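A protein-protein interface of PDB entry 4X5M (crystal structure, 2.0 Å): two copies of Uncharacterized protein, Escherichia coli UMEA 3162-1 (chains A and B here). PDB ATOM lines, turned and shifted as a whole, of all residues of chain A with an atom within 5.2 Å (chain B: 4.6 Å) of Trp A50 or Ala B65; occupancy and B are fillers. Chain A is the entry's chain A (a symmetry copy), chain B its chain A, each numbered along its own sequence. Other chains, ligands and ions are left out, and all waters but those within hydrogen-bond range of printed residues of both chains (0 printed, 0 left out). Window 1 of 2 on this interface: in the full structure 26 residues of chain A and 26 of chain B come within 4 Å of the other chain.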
ATOM      1  N   GLY A  46      20.805 -20.516 -13.744  1.00  0.00           N
ATOM      2  CA  GLY A  46      20.315 -19.953 -12.501  1.00  0.00           C
ATOM      3  C   GLY A  46      21.425 -19.354 -11.659  1.00  0.00           C
ATOM      4  O   GLY A  46      21.246 -18.299 -11.046  1.00  0.00           O
ATOM      5  N   VAL A  47      22.573 -20.028 -11.626  1.00  0.00           N
ATOM      6  CA  VAL A  47      23.727 -19.554 -10.864  1.00  0.00           C
ATOM      7  C   VAL A  47      24.184 -18.186 -11.358  1.00  0.00           C
ATOM      8  O   VAL A  47      24.426 -17.277 -10.562  1.00  0.00           O
ATOM      9  CB  VAL A  47      24.907 -20.547 -10.945  1.00  0.00           C
ATOM     10  CG1 VAL A  47      26.174 -19.921 -10.382  1.00  0.00           C
ATOM     11  CG2 VAL A  47      24.573 -21.831 -10.203  1.00  0.00           C
ATOM     12  N   ILE A  48      24.291 -18.046 -12.675  1.00  0.00           N
ATOM     13  CA  ILE A  48      24.638 -16.769 -13.290  1.00  0.00           C
ATOM     14  C   ILE A  48      23.619 -15.695 -12.913  1.00  0.00           C
ATOM     15  O   ILE A  48      23.983 -14.560 -12.601  1.00  0.00           O
ATOM     16  CB  ILE A  48      24.719 -16.889 -14.828  1.00  0.00           C
ATOM     17  CG1 ILE A  48      25.849 -17.838 -15.232  1.00  0.00           C
ATOM     18  CG2 ILE A  48      24.917 -15.525 -15.465  1.00  0.00           C
ATOM     19  CD1 ILE A  48      27.214 -17.421 -14.728  1.00  0.00           C
ATOM     20  N   SER A  49      22.344 -16.069 -12.926  1.00  0.00           N
ATOM     21  CA  SER A  49      21.270 -15.142 -12.588  1.00  0.00           C
ATOM     22  C   SER A  49      21.322 -14.728 -11.117  1.00  0.00           C
ATOM     23  O   SER A  49      21.009 -13.586 -10.778  1.00  0.00           O
ATOM     24  CB  SER A  49      19.910 -15.760 -12.920  1.00  0.00           C
ATOM     25  OG  SER A  49      19.810 -16.072 -14.299  1.00  0.00           O
ATOM     26  N   TRP A  50      21.712 -15.655 -10.245  1.00  0.00           N
ATOM     27  CA  TRP A  50      21.900 -15.335  -8.829  1.00  0.00           C
ATOM     28  C   TRP A  50      23.014 -14.312  -8.651  1.00  0.00           C
ATOM     29  O   TRP A  50      22.919 -13.416  -7.811  1.00  0.00           O
ATOM     30  CB  TRP A  50      22.224 -16.591  -8.015  1.00  0.00           C
ATOM     31  CG  TRP A  50      21.037 -17.411  -7.606  1.00  0.00           C
ATOM     32  CD1 TRP A  50      20.759 -18.690  -7.987  1.00  0.00           C
ATOM     33  CD2 TRP A  50      19.976 -17.016  -6.728  1.00  0.00           C
ATOM     34  NE1 TRP A  50      19.589 -19.115  -7.406  1.00  0.00           N
ATOM     35  CE2 TRP A  50      19.087 -18.102  -6.627  1.00  0.00           C
ATOM     36  CE3 TRP A  50      19.687 -15.844  -6.019  1.00  0.00           C
ATOM     37  CZ2 TRP A  50      17.933 -18.059  -5.849  1.00  0.00           C
ATOM     38  CZ3 TRP A  50      18.539 -15.800  -5.246  1.00  0.00           C
ATOM     39  CH2 TRP A  50      17.676 -16.900  -5.168  1.00  0.00           C
ATOM     40  N   ILE A  51      24.075 -14.463  -9.437  1.00  0.00           N
ATOM     41  CA  ILE A  51      25.205 -13.542  -9.388  1.00  0.00           C
ATOM     42  C   ILE A  51      24.763 -12.137  -9.784  1.00  0.00           C
ATOM     43  O   ILE A  51      25.115 -11.159  -9.125  1.00  0.00           O
ATOM     44  CB  ILE A  51      26.356 -14.009 -10.302  1.00  0.00           C
ATOM     45  CG1 ILE A  51      26.926 -15.335  -9.794  1.00  0.00           C
ATOM     46  CG2 ILE A  51      27.451 -12.956 -10.367  1.00  0.00           C
ATOM     47  CD1 ILE A  51      28.074 -15.872 -10.624  1.00  0.00           C
ATOM     48  N   ALA A  52      23.981 -12.044 -10.855  1.00  0.00           N
ATOM     49  CA  ALA A  52      23.402 -10.771 -11.268  1.00  0.00           C
ATOM     50  C   ALA A  52      22.502 -10.223 -10.167  1.00  0.00           C
ATOM     51  O   ALA A  52      22.527  -9.029  -9.863  1.00  0.00           O
ATOM     52  CB  ALA A  52      22.620 -10.932 -12.562  1.00  0.00           C
ATOM     53  N   TYR A  53      21.714 -11.112  -9.570  1.00  0.00           N
ATOM     54  CA  TYR A  53      20.823 -10.754  -8.474  1.00  0.00           C
ATOM     55  C   TYR A  53      21.609 -10.260  -7.266  1.00  0.00           C
ATOM     56  O   TYR A  53      21.259  -9.249  -6.659  1.00  0.00           O
ATOM     57  CB  TYR A  53      19.954 -11.949  -8.080  1.00  0.00           C
ATOM     58  CG  TYR A  53      18.906 -11.634  -7.037  1.00  0.00           C
ATOM     59  CD1 TYR A  53      17.870 -10.755  -7.316  1.00  0.00           C
ATOM     60  CD2 TYR A  53      18.944 -12.225  -5.779  1.00  0.00           C
ATOM     61  CE1 TYR A  53      16.904 -10.464  -6.374  1.00  0.00           C
ATOM     62  CE2 TYR A  53      17.980 -11.941  -4.827  1.00  0.00           C
ATOM     63  CZ  TYR A  53      16.961 -11.058  -5.132  1.00  0.00           C
ATOM     64  OH  TYR A  53      15.993 -10.763  -4.202  1.00  0.00           O
ATOM     65  N   GLY A  54      22.669 -10.985  -6.926  1.00  0.00           N
ATOM     66  CA  GLY A  54      23.518 -10.628  -5.804  1.00  0.00           C
ATOM     67  C   GLY A  54      24.162  -9.263  -5.959  1.00  0.00           C
ATOM     68  O   GLY A  54      24.284  -8.512  -4.992  1.00  0.00           O
ATOM     69  N   ILE A  55      24.575  -8.941  -7.181  1.00  0.00           N
ATOM     70  CA  ILE A  55      25.178  -7.644  -7.473  1.00  0.00           C
ATOM     71  C   ILE A  55      24.144  -6.534  -7.343  1.00  0.00           C
ATOM     72  O   ILE A  55      24.403  -5.490  -6.741  1.00  0.00           O
ATOM     73  CB  ILE A  55      25.791  -7.609  -8.889  1.00  0.00           C
ATOM     74  CG1 ILE A  55      26.990  -8.554  -8.975  1.00  0.00           C
ATOM     75  CG2 ILE A  55      26.206  -6.192  -9.260  1.00  0.00           C
ATOM     76  CD1 ILE A  55      27.579  -8.665 -10.367  1.00  0.00           C
ATOM     77  N   VAL A  62      24.964 -14.054  -1.081  1.00  0.00           N
ATOM     78  CA  VAL A  62      24.442 -14.659  -2.300  1.00  0.00           C
ATOM     79  C   VAL A  62      25.524 -14.712  -3.372  1.00  0.00           C
ATOM     80  O   VAL A  62      25.663 -15.709  -4.083  1.00  0.00           O
ATOM     81  CB  VAL A  62      23.218 -13.881  -2.831  1.00  0.00           C
ATOM     82  CG1 VAL A  62      22.832 -14.358  -4.223  1.00  0.00           C
ATOM     83  CG2 VAL A  62      22.045 -14.016  -1.868  1.00  0.00           C
ATOM     84  N   ASN A  66      27.321 -18.352  -4.969  1.00  0.00           N
ATOM     85  CA  ASN A  66      27.115 -18.760  -6.352  1.00  0.00           C
ATOM     86  C   ASN A  66      28.372 -18.655  -7.210  1.00  0.00           C
ATOM     87  O   ASN A  66      28.501 -19.354  -8.211  1.00  0.00           O
ATOM     88  CB  ASN A  66      25.991 -17.934  -6.974  1.00  0.00           C
ATOM     89  CG  ASN A  66      24.628 -18.318  -6.436  1.00  0.00           C
ATOM     90  OD1 ASN A  66      23.993 -19.248  -6.933  1.00  0.00           O
ATOM     91  ND2 ASN A  66      24.169 -17.603  -5.416  1.00  0.00           N
ATOM     92  N   GLY B   8      15.833 -12.556  -9.430  1.00  0.00           N
ATOM     93  CA  GLY B   8      16.003 -13.518  -8.356  1.00  0.00           C
ATOM     94  C   GLY B   8      15.071 -14.706  -8.497  1.00  0.00           C
ATOM     95  O   GLY B   8      15.470 -15.850  -8.275  1.00  0.00           O
ATOM     96  N   ALA B  11      16.326 -16.772 -11.205  1.00  0.00           N
ATOM     97  CA  ALA B  11      17.426 -17.562 -10.671  1.00  0.00           C
ATOM     98  C   ALA B  11      16.917 -18.707  -9.805  1.00  0.00           C
ATOM     99  O   ALA B  11      17.379 -19.842  -9.927  1.00  0.00           O
ATOM    100  CB  ALA B  11      18.368 -16.677  -9.868  1.00  0.00           C
ATOM    101  N   ALA B  12      15.967 -18.394  -8.928  1.00  0.00           N
ATOM    102  CA  ALA B  12      15.399 -19.383  -8.019  1.00  0.00           C
ATOM    103  C   ALA B  12      14.738 -20.527  -8.779  1.00  0.00           C
ATOM    104  O   ALA B  12      14.855 -21.686  -8.387  1.00  0.00           O
ATOM    105  CB  ALA B  12      14.398 -18.722  -7.080  1.00  0.00           C
ATOM    106  N   THR B  15      17.763 -22.839 -10.498  1.00  0.00           N
ATOM    107  CA  THR B  15      18.625 -23.575  -9.576  1.00  0.00           C
ATOM    108  C   THR B  15      17.853 -24.597  -8.746  1.00  0.00           C
ATOM    109  O   THR B  15      18.390 -25.648  -8.393  1.00  0.00           O
ATOM    110  CB  THR B  15      19.378 -22.632  -8.614  1.00  0.00           C
ATOM    111  OG1 THR B  15      18.444 -21.784  -7.936  1.00  0.00           O
ATOM    112  CG2 THR B  15      20.375 -21.784  -9.379  1.00  0.00           C
ATOM    113  N   THR B  16      16.595 -24.296  -8.435  1.00  0.00           N
ATOM    114  CA  THR B  16      15.801 -25.190  -7.596  1.00  0.00           C
ATOM    115  C   THR B  16      15.256 -26.377  -8.386  1.00  0.00           C
ATOM    116  O   THR B  16      15.236 -27.504  -7.891  1.00  0.00           O
ATOM    117  CB  THR B  16      14.622 -24.453  -6.928  1.00  0.00           C
ATOM    118  OG1 THR B  16      15.099 -23.268  -6.278  1.00  0.00           O
ATOM    119  CG2 THR B  16      13.949 -25.346  -5.899  1.00  0.00           C
ATOM    120  N   ALA B  61      13.029 -13.988  -3.121  1.00  0.00           N
ATOM    121  CA  ALA B  61      13.715 -14.872  -4.055  1.00  0.00           C
ATOM    122  C   ALA B  61      14.529 -15.914  -3.297  1.00  0.00           C
ATOM    123  O   ALA B  61      14.438 -17.110  -3.571  1.00  0.00           O
ATOM    124  CB  ALA B  61      14.609 -14.074  -4.990  1.00  0.00           C
ATOM    125  N   VAL B  62      15.322 -15.448  -2.337  1.00  0.00           N
ATOM    126  CA  VAL B  62      16.107 -16.332  -1.486  1.00  0.00           C
ATOM    127  C   VAL B  62      15.189 -17.210  -0.644  1.00  0.00           C
ATOM    128  O   VAL B  62      15.438 -18.405  -0.473  1.00  0.00           O
ATOM    129  CB  VAL B  62      17.052 -15.529  -0.565  1.00  0.00           C
ATOM    130  CG1 VAL B  62      17.681 -16.429   0.488  1.00  0.00           C
ATOM    131  CG2 VAL B  62      18.124 -14.827  -1.388  1.00  0.00           C
ATOM    132  N   LEU B  63      14.118 -16.608  -0.135  1.00  0.00           N
ATOM    133  CA  LEU B  63      13.154 -17.310   0.706  1.00  0.00           C
ATOM    134  C   LEU B  63      12.507 -18.499   0.003  1.00  0.00           C
ATOM    135  O   LEU B  63      12.631 -19.635   0.461  1.00  0.00           O
ATOM    136  CB  LEU B  63      12.068 -16.346   1.187  1.00  0.00           C
ATOM    137  CG  LEU B  63      12.243 -15.786   2.599  1.00  0.00           C
ATOM    138  CD1 LEU B  63      11.089 -14.863   2.963  1.00  0.00           C
ATOM    139  CD2 LEU B  63      12.363 -16.921   3.605  1.00  0.00           C
ATOM    140  N   ILE B  64      11.819 -18.238  -1.105  1.00  0.00           N
ATOM    141  CA  ILE B  64      11.070 -19.284  -1.795  1.00  0.00           C
ATOM    142  C   ILE B  64      11.996 -20.358  -2.365  1.00  0.00           C
ATOM    143  O   ILE B  64      11.615 -21.523  -2.462  1.00  0.00           O
ATOM    144  CB  ILE B  64      10.183 -18.701  -2.928  1.00  0.00           C
ATOM    145  CG1 ILE B  64       9.166 -19.740  -3.408  1.00  0.00           C
ATOM    146  CG2 ILE B  64      11.032 -18.187  -4.088  1.00  0.00           C
ATOM    147  CD1 ILE B  64       8.264 -19.245  -4.519  1.00  0.00           C
ATOM    148  N   ALA B  65      13.218 -19.972  -2.719  1.00  0.00           N
ATOM    149  CA  ALA B  65      14.184 -20.916  -3.266  1.00  0.00           C
ATOM    150  C   ALA B  65      14.542 -21.981  -2.236  1.00  0.00           C
ATOM    151  O   ALA B  65      14.569 -23.174  -2.541  1.00  0.00           O
ATOM    152  CB  ALA B  65      15.436 -20.187  -3.731  1.00  0.00           C
ATOM    153  N   ASN B  66      14.800 -21.539  -1.011  1.00  0.00           N
ATOM    154  CA  ASN B  66      15.236 -22.436   0.051  1.00  0.00           C
ATOM    155  C   ASN B  66      14.086 -23.143   0.760  1.00  0.00           C
ATOM    156  O   ASN B  66      14.270 -24.218   1.324  1.00  0.00           O
ATOM    157  CB  ASN B  66      16.079 -21.667   1.066  1.00  0.00           C
ATOM    158  CG  ASN B  66      17.445 -21.302   0.523  1.00  0.00           C
ATOM    159  OD1 ASN B  66      18.384 -22.095   0.595  1.00  0.00           O
ATOM    160  ND2 ASN B  66      17.565 -20.098  -0.024  1.00  0.00           N
ATOM    161  N   ILE B  67      12.899 -22.542   0.735  1.00  0.00           N
ATOM    162  CA  ILE B  67      11.728 -23.195   1.308  1.00  0.00           C
ATOM    163  C   ILE B  67      11.353 -24.404   0.456  1.00  0.00           C
ATOM    164  O   ILE B  67      11.089 -25.485   0.982  1.00  0.00           O
ATOM    165  CB  ILE B  67      10.526 -22.235   1.423  1.00  0.00           C
ATOM    166  CG1 ILE B  67      10.782 -21.196   2.515  1.00  0.00           C
ATOM    167  CG2 ILE B  67       9.254 -23.008   1.738  1.00  0.00           C
ATOM    168  CD1 ILE B  67       9.707 -20.133   2.618  1.00  0.00           C
ATOM    169  N   VAL B  68      11.347 -24.219  -0.862  1.00  0.00           N
ATOM    170  CA  VAL B  68      11.090 -25.321  -1.784  1.00  0.00           C
ATOM    171  C   VAL B  68      12.191 -26.374  -1.669  1.00  0.00           C
ATOM    172  O   VAL B  68      11.916 -27.577  -1.670  1.00  0.00           O
ATOM    173  CB  VAL B  68      10.990 -24.835  -3.248  1.00  0.00           C
ATOM    174  CG1 VAL B  68      10.851 -26.016  -4.194  1.00  0.00           C
ATOM    175  CG2 VAL B  68       9.816 -23.889  -3.413  1.00  0.00           C
ATOM    176  N   THR B  69      13.433 -25.911  -1.558  1.00  0.00           N
ATOM    177  CA  THR B  69      14.573 -26.800  -1.346  1.00  0.00           C
ATOM    178  C   THR B  69      14.375 -27.630  -0.081  1.00  0.00           C
ATOM    179  O   THR B  69      14.654 -28.830  -0.064  1.00  0.00           O
ATOM    180  CB  THR B  69      15.896 -26.012  -1.237  1.00  0.00           C
ATOM    181  OG1 THR B  69      16.135 -25.304  -2.459  1.00  0.00           O
ATOM    182  CG2 THR B  69      17.061 -26.950  -0.974  1.00  0.00           C
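2 positions are printed for both chains.
The backbone carbonyl oxygen of Ala B11 is in hydrogen-bond range of the indole nitrogen of Trp A50, 3.4 Å away.
The indole nitrogen (NE1) of Trp A50 is in hydrogen-bond range of the side-chain hydroxyl (OG1) of Thr B15 (3.0 Å).
Gly A46 touches Ala B11 (O to CB, 3.5 Å).
Gly A46 touches Thr B15.
Val A47 touches Thr B15 (N to CG2, 3.6 Å).
Ala B11 touches Ser A49.
Trp A50 touches Gly B8.
CZ2 of Trp A50 touches CA of Ala B12, at 3.6 Å.
Trp A50 touches Val B62 (CH2 to N, 3.96 Å).
Trp A50 touches Ala B65.
Tyr A53 touches Gly B8.
Tyr A53 touches Ala B61 (OH to CB, 3.7 Å).
Printed residues of chain B within 4 Å of Gly A46: Ala B11 (3.5 Å) and Thr B15 (3.5 Å).
Trp A50 touches just these residues of chain B: Gly B8 (3.95 Å), Ala B11 (3.4 Å), Ala B12 (3.6 Å), Thr B15 (3.0 Å), Ala B61 (3.6 Å), Val B62 (3.96 Å) and Ala B65 (3.9 Å).
Of the printed residues of chain A, Ala B12 touches Trp A50.
Printed residues of chain A within 4 Å of Ala B61: Trp A50 and Tyr A53.
Ala B65 touches just one residue of chain A: Trp A50.
The nearest printed residue of chain A that does not touch Ala B65 is Tyr A53 (8.7 Å).
Printed residues of chain A that touch a printed residue of chain B: Gly A46, Val A47, Ser A49, Trp A50 and Tyr A53.
Of the 14 printed residues of chain B, 7 touch a printed residue of chain A.
Printed residues of chain B that touch a printed residue of chain A: Gly B8, Ala B11, Ala B12, Thr B15, Ala B61, Val B62 and Ala B65.
Hydrophobic or aromatic side chains of chain B that line the printed part of chain A: Ala B11, Ala B12, Ala B61 and Ala B65.
Among the printed residues, 13 pairs touch across the chains.
Among the printed residues, no Asp or Glu carboxylate lies within 4 Å of a Lys or Arg side-chain nitrogen of the other chain.
O of Ala B11 is in hydrogen-bond range of OG1 of Thr B15 (3.0 Å).
The backbone carbonyl oxygen (O) of Ala B12 lies within hydrogen-bond range of the side-chain hydroxyl (OG1) of Thr B16 (2.6 Å).
ND2 of Asn B66 sits at hydrogen-bond distance from O of Val B62 (2.8 Å).
OG1 of Thr B69 sits at hydrogen-bond distance from O of Ala B65 (2.6 Å).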
